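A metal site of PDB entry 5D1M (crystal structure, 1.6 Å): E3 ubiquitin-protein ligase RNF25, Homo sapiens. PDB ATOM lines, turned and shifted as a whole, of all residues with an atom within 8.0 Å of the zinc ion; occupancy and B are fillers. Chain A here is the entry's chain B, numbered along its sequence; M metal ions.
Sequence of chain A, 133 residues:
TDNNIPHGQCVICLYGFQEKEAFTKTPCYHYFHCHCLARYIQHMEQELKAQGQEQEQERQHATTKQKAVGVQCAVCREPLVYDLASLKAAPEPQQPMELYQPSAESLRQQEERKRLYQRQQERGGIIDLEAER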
ATOM      1  N   GLN A   9     -11.741  -4.145 -30.012  1.00  0.00           N
ATOM      2  CA  GLN A   9     -12.205  -2.793 -29.717  1.00  0.00           C
ATOM      3  C   GLN A   9     -11.678  -2.276 -28.386  1.00  0.00           C
ATOM      4  O   GLN A   9     -11.340  -3.058 -27.483  1.00  0.00           O
ATOM      5  CB  GLN A   9     -13.734  -2.718 -29.744  1.00  0.00           C
ATOM      6  CG  GLN A   9     -14.336  -2.219 -31.051  1.00  0.00           C
ATOM      7  CD  GLN A   9     -14.088  -3.148 -32.217  1.00  0.00           C
ATOM      8  OE1 GLN A   9     -13.612  -2.732 -33.273  1.00  0.00           O
ATOM      9  NE2 GLN A   9     -14.410  -4.427 -32.041  1.00  0.00           N
ATOM     10  N   CYS A  10     -11.571  -0.954 -28.270  1.00  0.00           N
ATOM     11  CA  CYS A  10     -11.248  -0.303 -26.995  1.00  0.00           C
ATOM     12  C   CYS A  10     -12.582  -0.166 -26.230  1.00  0.00           C
ATOM     13  O   CYS A  10     -13.487   0.478 -26.741  1.00  0.00           O
ATOM     14  CB  CYS A  10     -10.686   1.105 -27.271  1.00  0.00           C
ATOM     15  SG  CYS A  10     -10.394   2.102 -25.791  1.00  0.00           S
ATOM     16  N   VAL A  11     -12.727  -0.767 -25.038  1.00  0.00           N
ATOM     17  CA  VAL A  11     -14.054  -0.747 -24.367  1.00  0.00           C
ATOM     18  C   VAL A  11     -14.435   0.610 -23.783  1.00  0.00           C
ATOM     19  O   VAL A  11     -15.597   0.830 -23.423  1.00  0.00           O
ATOM     20  CB  VAL A  11     -14.201  -1.817 -23.234  1.00  0.00           C
ATOM     21  CG1 VAL A  11     -14.087  -3.219 -23.802  1.00  0.00           C
ATOM     22  CG2 VAL A  11     -13.174  -1.585 -22.111  1.00  0.00           C
ATOM     23  N   ILE A  12     -13.466   1.520 -23.673  1.00  0.00           N
ATOM     24  CA  ILE A  12     -13.749   2.865 -23.180  1.00  0.00           C
ATOM     25  C   ILE A  12     -14.466   3.714 -24.228  1.00  0.00           C
ATOM     26  O   ILE A  12     -15.504   4.319 -23.924  1.00  0.00           O
ATOM     27  CB  ILE A  12     -12.486   3.561 -22.616  1.00  0.00           C
ATOM     28  CG1 ILE A  12     -12.002   2.790 -21.389  1.00  0.00           C
ATOM     29  CG2 ILE A  12     -12.777   5.011 -22.276  1.00  0.00           C
ATOM     30  CD1 ILE A  12     -10.582   3.190 -20.928  1.00  0.00           C
ATOM     31  N   CYS A  13     -13.936   3.752 -25.471  1.00  0.00           N
ATOM     32  CA  CYS A  13     -14.514   4.574 -26.552  1.00  0.00           C
ATOM     33  C   CYS A  13     -15.437   3.810 -27.543  1.00  0.00           C
ATOM     34  O   CYS A  13     -16.209   4.443 -28.293  1.00  0.00           O
ATOM     35  CB  CYS A  13     -13.438   5.325 -27.343  1.00  0.00           C
ATOM     36  SG  CYS A  13     -12.353   4.261 -28.394  1.00  0.00           S
ATOM     37  N   LEU A  14     -15.296   2.489 -27.575  1.00  0.00           N
ATOM     38  CA  LEU A  14     -16.037   1.581 -28.477  1.00  0.00           C
ATOM     39  C   LEU A  14     -15.589   1.612 -29.955  1.00  0.00           C
ATOM     40  O   LEU A  14     -16.295   1.101 -30.818  1.00  0.00           O
ATOM     41  CB  LEU A  14     -17.571   1.781 -28.355  1.00  0.00           C
ATOM     42  CG  LEU A  14     -18.129   1.589 -26.932  1.00  0.00           C
ATOM     43  CD1 LEU A  14     -19.650   1.910 -26.847  1.00  0.00           C
ATOM     44  CD2 LEU A  14     -17.848   0.211 -26.387  1.00  0.00           C
ATOM     45  N   TYR A  15     -14.410   2.180 -30.237  1.00  0.00           N
ATOM     46  CA  TYR A  15     -13.814   2.127 -31.584  1.00  0.00           C
ATOM     47  C   TYR A  15     -12.675   1.096 -31.618  1.00  0.00           C
ATOM     48  O   TYR A  15     -12.111   0.728 -30.581  1.00  0.00           O
ATOM     49  CB  TYR A  15     -13.260   3.490 -32.013  1.00  0.00           C
ATOM     50  CG  TYR A  15     -14.268   4.586 -32.367  1.00  0.00           C
ATOM     51  CD1 TYR A  15     -14.972   5.258 -31.378  1.00  0.00           C
ATOM     52  CD2 TYR A  15     -14.463   4.981 -33.691  1.00  0.00           C
ATOM     53  CE1 TYR A  15     -15.876   6.256 -31.683  1.00  0.00           C
ATOM     54  CE2 TYR A  15     -15.372   5.999 -34.008  1.00  0.00           C
ATOM     55  CZ  TYR A  15     -16.076   6.631 -32.998  1.00  0.00           C
ATOM     56  OH  TYR A  15     -16.978   7.648 -33.280  1.00  0.00           O
ATOM     57  N   GLY A  16     -12.332   0.643 -32.829  1.00  0.00           N
ATOM     58  CA  GLY A  16     -11.212  -0.260 -33.041  1.00  0.00           C
ATOM     59  C   GLY A  16      -9.882   0.466 -33.211  1.00  0.00           C
ATOM     60  O   GLY A  16      -9.753   1.662 -32.926  1.00  0.00           O
ATOM     61  N   PHE A  17      -8.872  -0.273 -33.666  1.00  0.00           N
ATOM     62  CA  PHE A  17      -7.527   0.270 -33.768  1.00  0.00           C
ATOM     63  C   PHE A  17      -7.067   0.399 -35.229  1.00  0.00           C
ATOM     64  O   PHE A  17      -7.413  -0.434 -36.086  1.00  0.00           O
ATOM     65  CB  PHE A  17      -6.546  -0.569 -32.930  1.00  0.00           C
ATOM     66  CG  PHE A  17      -6.948  -0.692 -31.478  1.00  0.00           C
ATOM     67  CD1 PHE A  17      -6.637   0.323 -30.580  1.00  0.00           C
ATOM     68  CD2 PHE A  17      -7.655  -1.806 -31.020  1.00  0.00           C
ATOM     69  CE1 PHE A  17      -7.008   0.222 -29.234  1.00  0.00           C
ATOM     70  CE2 PHE A  17      -8.032  -1.906 -29.687  1.00  0.00           C
ATOM     71  CZ  PHE A  17      -7.707  -0.882 -28.794  1.00  0.00           C
ATOM     72  N   GLU A  21      -2.505   5.121 -35.199  1.00  0.00           N
ATOM     73  CA  GLU A  21      -3.062   5.413 -33.879  1.00  0.00           C
ATOM     74  C   GLU A  21      -2.128   4.989 -32.754  1.00  0.00           C
ATOM     75  O   GLU A  21      -1.378   4.015 -32.883  1.00  0.00           O
ATOM     76  CB  GLU A  21      -4.417   4.718 -33.696  1.00  0.00           C
ATOM     77  CG  GLU A  21      -5.547   5.353 -34.465  1.00  0.00           C
ATOM     78  CD  GLU A  21      -6.872   4.703 -34.153  1.00  0.00           C
ATOM     79  OE1 GLU A  21      -6.887   3.630 -33.505  1.00  0.00           O
ATOM     80  OE2 GLU A  21      -7.911   5.260 -34.556  1.00  0.00           O
ATOM     81  N   ALA A  22      -2.177   5.749 -31.664  1.00  0.00           N
ATOM     82  CA  ALA A  22      -1.446   5.444 -30.434  1.00  0.00           C
ATOM     83  C   ALA A  22      -2.318   4.634 -29.458  1.00  0.00           C
ATOM     84  O   ALA A  22      -3.337   5.111 -28.944  1.00  0.00           O
ATOM     85  CB  ALA A  22      -0.972   6.727 -29.770  1.00  0.00           C
ATOM     86  N   PHE A  23      -1.899   3.397 -29.191  1.00  0.00           N
ATOM     87  CA  PHE A  23      -2.642   2.521 -28.283  1.00  0.00           C
ATOM     88  C   PHE A  23      -1.652   1.712 -27.463  1.00  0.00           C
ATOM     89  O   PHE A  23      -0.461   1.671 -27.810  1.00  0.00           O
ATOM     90  CB  PHE A  23      -3.588   1.591 -29.049  1.00  0.00           C
ATOM     91  CG  PHE A  23      -2.915   0.803 -30.148  1.00  0.00           C
ATOM     92  CD1 PHE A  23      -2.240  -0.380 -29.868  1.00  0.00           C
ATOM     93  CD2 PHE A  23      -2.982   1.231 -31.465  1.00  0.00           C
ATOM     94  CE1 PHE A  23      -1.627  -1.106 -30.882  1.00  0.00           C
ATOM     95  CE2 PHE A  23      -2.369   0.504 -32.479  1.00  0.00           C
ATOM     96  CZ  PHE A  23      -1.696  -0.659 -32.190  1.00  0.00           C
ATOM     97  N   TYR A  31      -6.337  -4.143 -24.466  1.00  0.00           N
ATOM     98  CA  TYR A  31      -5.876  -3.002 -25.286  1.00  0.00           C
ATOM     99  C   TYR A  31      -6.791  -1.789 -25.101  1.00  0.00           C
ATOM    100  O   TYR A  31      -8.027  -1.914 -25.092  1.00  0.00           O
ATOM    101  CB  TYR A  31      -5.841  -3.366 -26.797  1.00  0.00           C
ATOM    102  CG  TYR A  31      -4.763  -4.360 -27.228  1.00  0.00           C
ATOM    103  CD1 TYR A  31      -4.974  -5.723 -27.160  1.00  0.00           C
ATOM    104  CD2 TYR A  31      -3.543  -3.908 -27.721  1.00  0.00           C
ATOM    105  CE1 TYR A  31      -3.985  -6.612 -27.561  1.00  0.00           C
ATOM    106  CE2 TYR A  31      -2.553  -4.777 -28.121  1.00  0.00           C
ATOM    107  CZ  TYR A  31      -2.778  -6.139 -28.048  1.00  0.00           C
ATOM    108  OH  TYR A  31      -1.792  -7.019 -28.439  1.00  0.00           O
ATOM    109  N   PHE A  32      -6.175  -0.618 -24.973  1.00  0.00           N
ATOM    110  CA  PHE A  32      -6.919   0.659 -24.914  1.00  0.00           C
ATOM    111  C   PHE A  32      -6.166   1.702 -25.730  1.00  0.00           C
ATOM    112  O   PHE A  32      -4.942   1.630 -25.830  1.00  0.00           O
ATOM    113  CB  PHE A  32      -7.014   1.139 -23.447  1.00  0.00           C
ATOM    114  CG  PHE A  32      -7.638   0.133 -22.485  1.00  0.00           C
ATOM    115  CD1 PHE A  32      -9.008   0.120 -22.270  1.00  0.00           C
ATOM    116  CD2 PHE A  32      -6.839  -0.761 -21.770  1.00  0.00           C
ATOM    117  CE1 PHE A  32      -9.585  -0.796 -21.385  1.00  0.00           C
ATOM    118  CE2 PHE A  32      -7.406  -1.667 -20.881  1.00  0.00           C
ATOM    119  CZ  PHE A  32      -8.782  -1.689 -20.679  1.00  0.00           C
ATOM    120  N   HIS A  33      -6.864   2.685 -26.299  1.00  0.00           N
ATOM    121  CA  HIS A  33      -6.138   3.850 -26.824  1.00  0.00           C
ATOM    122  C   HIS A  33      -5.487   4.523 -25.617  1.00  0.00           C
ATOM    123  O   HIS A  33      -6.011   4.509 -24.500  1.00  0.00           O
ATOM    124  CB  HIS A  33      -7.056   4.833 -27.574  1.00  0.00           C
ATOM    125  CG  HIS A  33      -7.690   4.269 -28.806  1.00  0.00           C
ATOM    126  ND1 HIS A  33      -8.986   3.768 -28.824  1.00  0.00           N
ATOM    127  CD2 HIS A  33      -7.213   4.090 -30.060  1.00  0.00           C
ATOM    128  CE1 HIS A  33      -9.264   3.313 -30.037  1.00  0.00           C
ATOM    129  NE2 HIS A  33      -8.196   3.493 -30.805  1.00  0.00           N
ATOM    130  N   CYS A  34      -4.304   5.099 -25.823  1.00  0.00           N
ATOM    131  CA  CYS A  34      -3.599   5.712 -24.713  1.00  0.00           C
ATOM    132  C   CYS A  34      -4.411   6.854 -24.082  1.00  0.00           C
ATOM    133  O   CYS A  34      -4.482   6.999 -22.855  1.00  0.00           O
ATOM    134  CB  CYS A  34      -2.240   6.226 -25.195  1.00  0.00           C
ATOM    135  SG  CYS A  34      -1.146   4.841 -25.657  1.00  0.00           S
ATOM    136  N   HIS A  35      -5.041   7.642 -24.948  1.00  0.00           N
ATOM    137  CA  HIS A  35      -5.885   8.742 -24.522  1.00  0.00           C
ATOM    138  C   HIS A  35      -7.059   8.265 -23.647  1.00  0.00           C
ATOM    139  O   HIS A  35      -7.338   8.829 -22.582  1.00  0.00           O
ATOM    140  CB  HIS A  35      -6.392   9.465 -25.780  1.00  0.00           C
ATOM    141  CG  HIS A  35      -7.374  10.539 -25.503  1.00  0.00           C
ATOM    142  ND1 HIS A  35      -7.010  11.807 -25.117  1.00  0.00           N
ATOM    143  CD2 HIS A  35      -8.729  10.543 -25.550  1.00  0.00           C
ATOM    144  CE1 HIS A  35      -8.093  12.550 -24.947  1.00  0.00           C
ATOM    145  NE2 HIS A  35      -9.157  11.801 -25.199  1.00  0.00           N
ATOM    146  N   CYS A  36      -7.709   7.196 -24.087  1.00  0.00           N
ATOM    147  CA  CYS A  36      -8.847   6.640 -23.350  1.00  0.00           C
ATOM    148  C   CYS A  36      -8.474   6.141 -21.948  1.00  0.00           C
ATOM    149  O   CYS A  36      -9.166   6.402 -20.958  1.00  0.00           O
ATOM    150  CB  CYS A  36      -9.454   5.501 -24.170  1.00  0.00           C
ATOM    151  SG  CYS A  36     -10.148   6.095 -25.725  1.00  0.00           S
ATOM    152  N   LEU A  37      -7.364   5.409 -21.851  1.00  0.00           N
ATOM    153  CA  LEU A  37      -6.925   4.860 -20.575  1.00  0.00           C
ATOM    154  C   LEU A  37      -6.499   5.955 -19.599  1.00  0.00           C
ATOM    155  O   LEU A  37      -6.727   5.850 -18.403  1.00  0.00           O
ATOM    156  CB  LEU A  37      -5.805   3.816 -20.788  1.00  0.00           C
ATOM    157  CG  LEU A  37      -5.350   3.056 -19.539  1.00  0.00           C
ATOM    158  CD1 LEU A  37      -6.527   2.218 -18.979  1.00  0.00           C
ATOM    159  CD2 LEU A  37      -4.185   2.144 -19.873  1.00  0.00           C
ATOM    160  N   PRO A  93      -6.915   9.763 -30.902  1.00  0.00           N
ATOM    161  CA  PRO A  93      -7.325   9.188 -32.188  1.00  0.00           C
ATOM    162  C   PRO A  93      -8.398  10.027 -32.869  1.00  0.00           C
ATOM    163  O   PRO A  93      -9.286  10.540 -32.187  1.00  0.00           O
ATOM    164  CB  PRO A  93      -7.931   7.829 -31.789  1.00  0.00           C
ATOM    165  CG  PRO A  93      -7.390   7.542 -30.450  1.00  0.00           C
ATOM    166  CD  PRO A  93      -7.175   8.850 -29.778  1.00  0.00           C
ATOM    167  N   GLN A  95     -11.571  10.044 -34.842  1.00  0.00           N
ATOM    168  CA  GLN A  95     -12.646   9.094 -35.047  1.00  0.00           C
ATOM    169  C   GLN A  95     -13.915   9.854 -35.398  1.00  0.00           C
ATOM    170  O   GLN A  95     -14.489  10.534 -34.551  1.00  0.00           O
ATOM    171  CB  GLN A  95     -12.849   8.273 -33.773  1.00  0.00           C
ATOM    172  CG  GLN A  95     -11.556   7.695 -33.198  1.00  0.00           C
ATOM    173  CD  GLN A  95     -11.707   7.197 -31.772  1.00  0.00           C
ATOM    174  OE1 GLN A  95     -12.195   7.900 -30.892  1.00  0.00           O
ATOM    175  NE2 GLN A  95     -11.255   5.969 -31.535  1.00  0.00           N
HETATM  176 ZN    ZN M   1     -10.465   4.113 -27.074  1.00  0.00          ZN
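SG of Cys 10 sits close to N of Ile 12. SG of Cys 13 sits close to N of Tyr 15 (3.5 Å). The backbone carbonyl oxygen (O) of Tyr 15 lies within hydrogen-bond range of the backbone NH (N) of Cys 10 (2.9 Å). The backbone carbonyl oxygen of Gly 16 is in hydrogen-bond range of a ring nitrogen (NE2) of His 33. NE2 of Gln 95 lies close to SG of Cys 13, 3.7 Å away. The side-chain carboxylate of Glu 21 lies within hydrogen-bond range of a ring nitrogen (NE2) of His 33 (3.0 Å).
The nearest printed residue that does not touch the zinc ion is Gln 95 (4.9 Å).
The zinc ion is bound by the side-chain sulfur of Cys 13 (2.3 Å), a ring nitrogen (ND1) of His 33 (2.3 Å), the side-chain sulfur of Cys 10 (2.4 Å) and the side-chain sulfur of Cys 36 (2.4 Å). The zinc ion has four donor atoms within binding distance.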
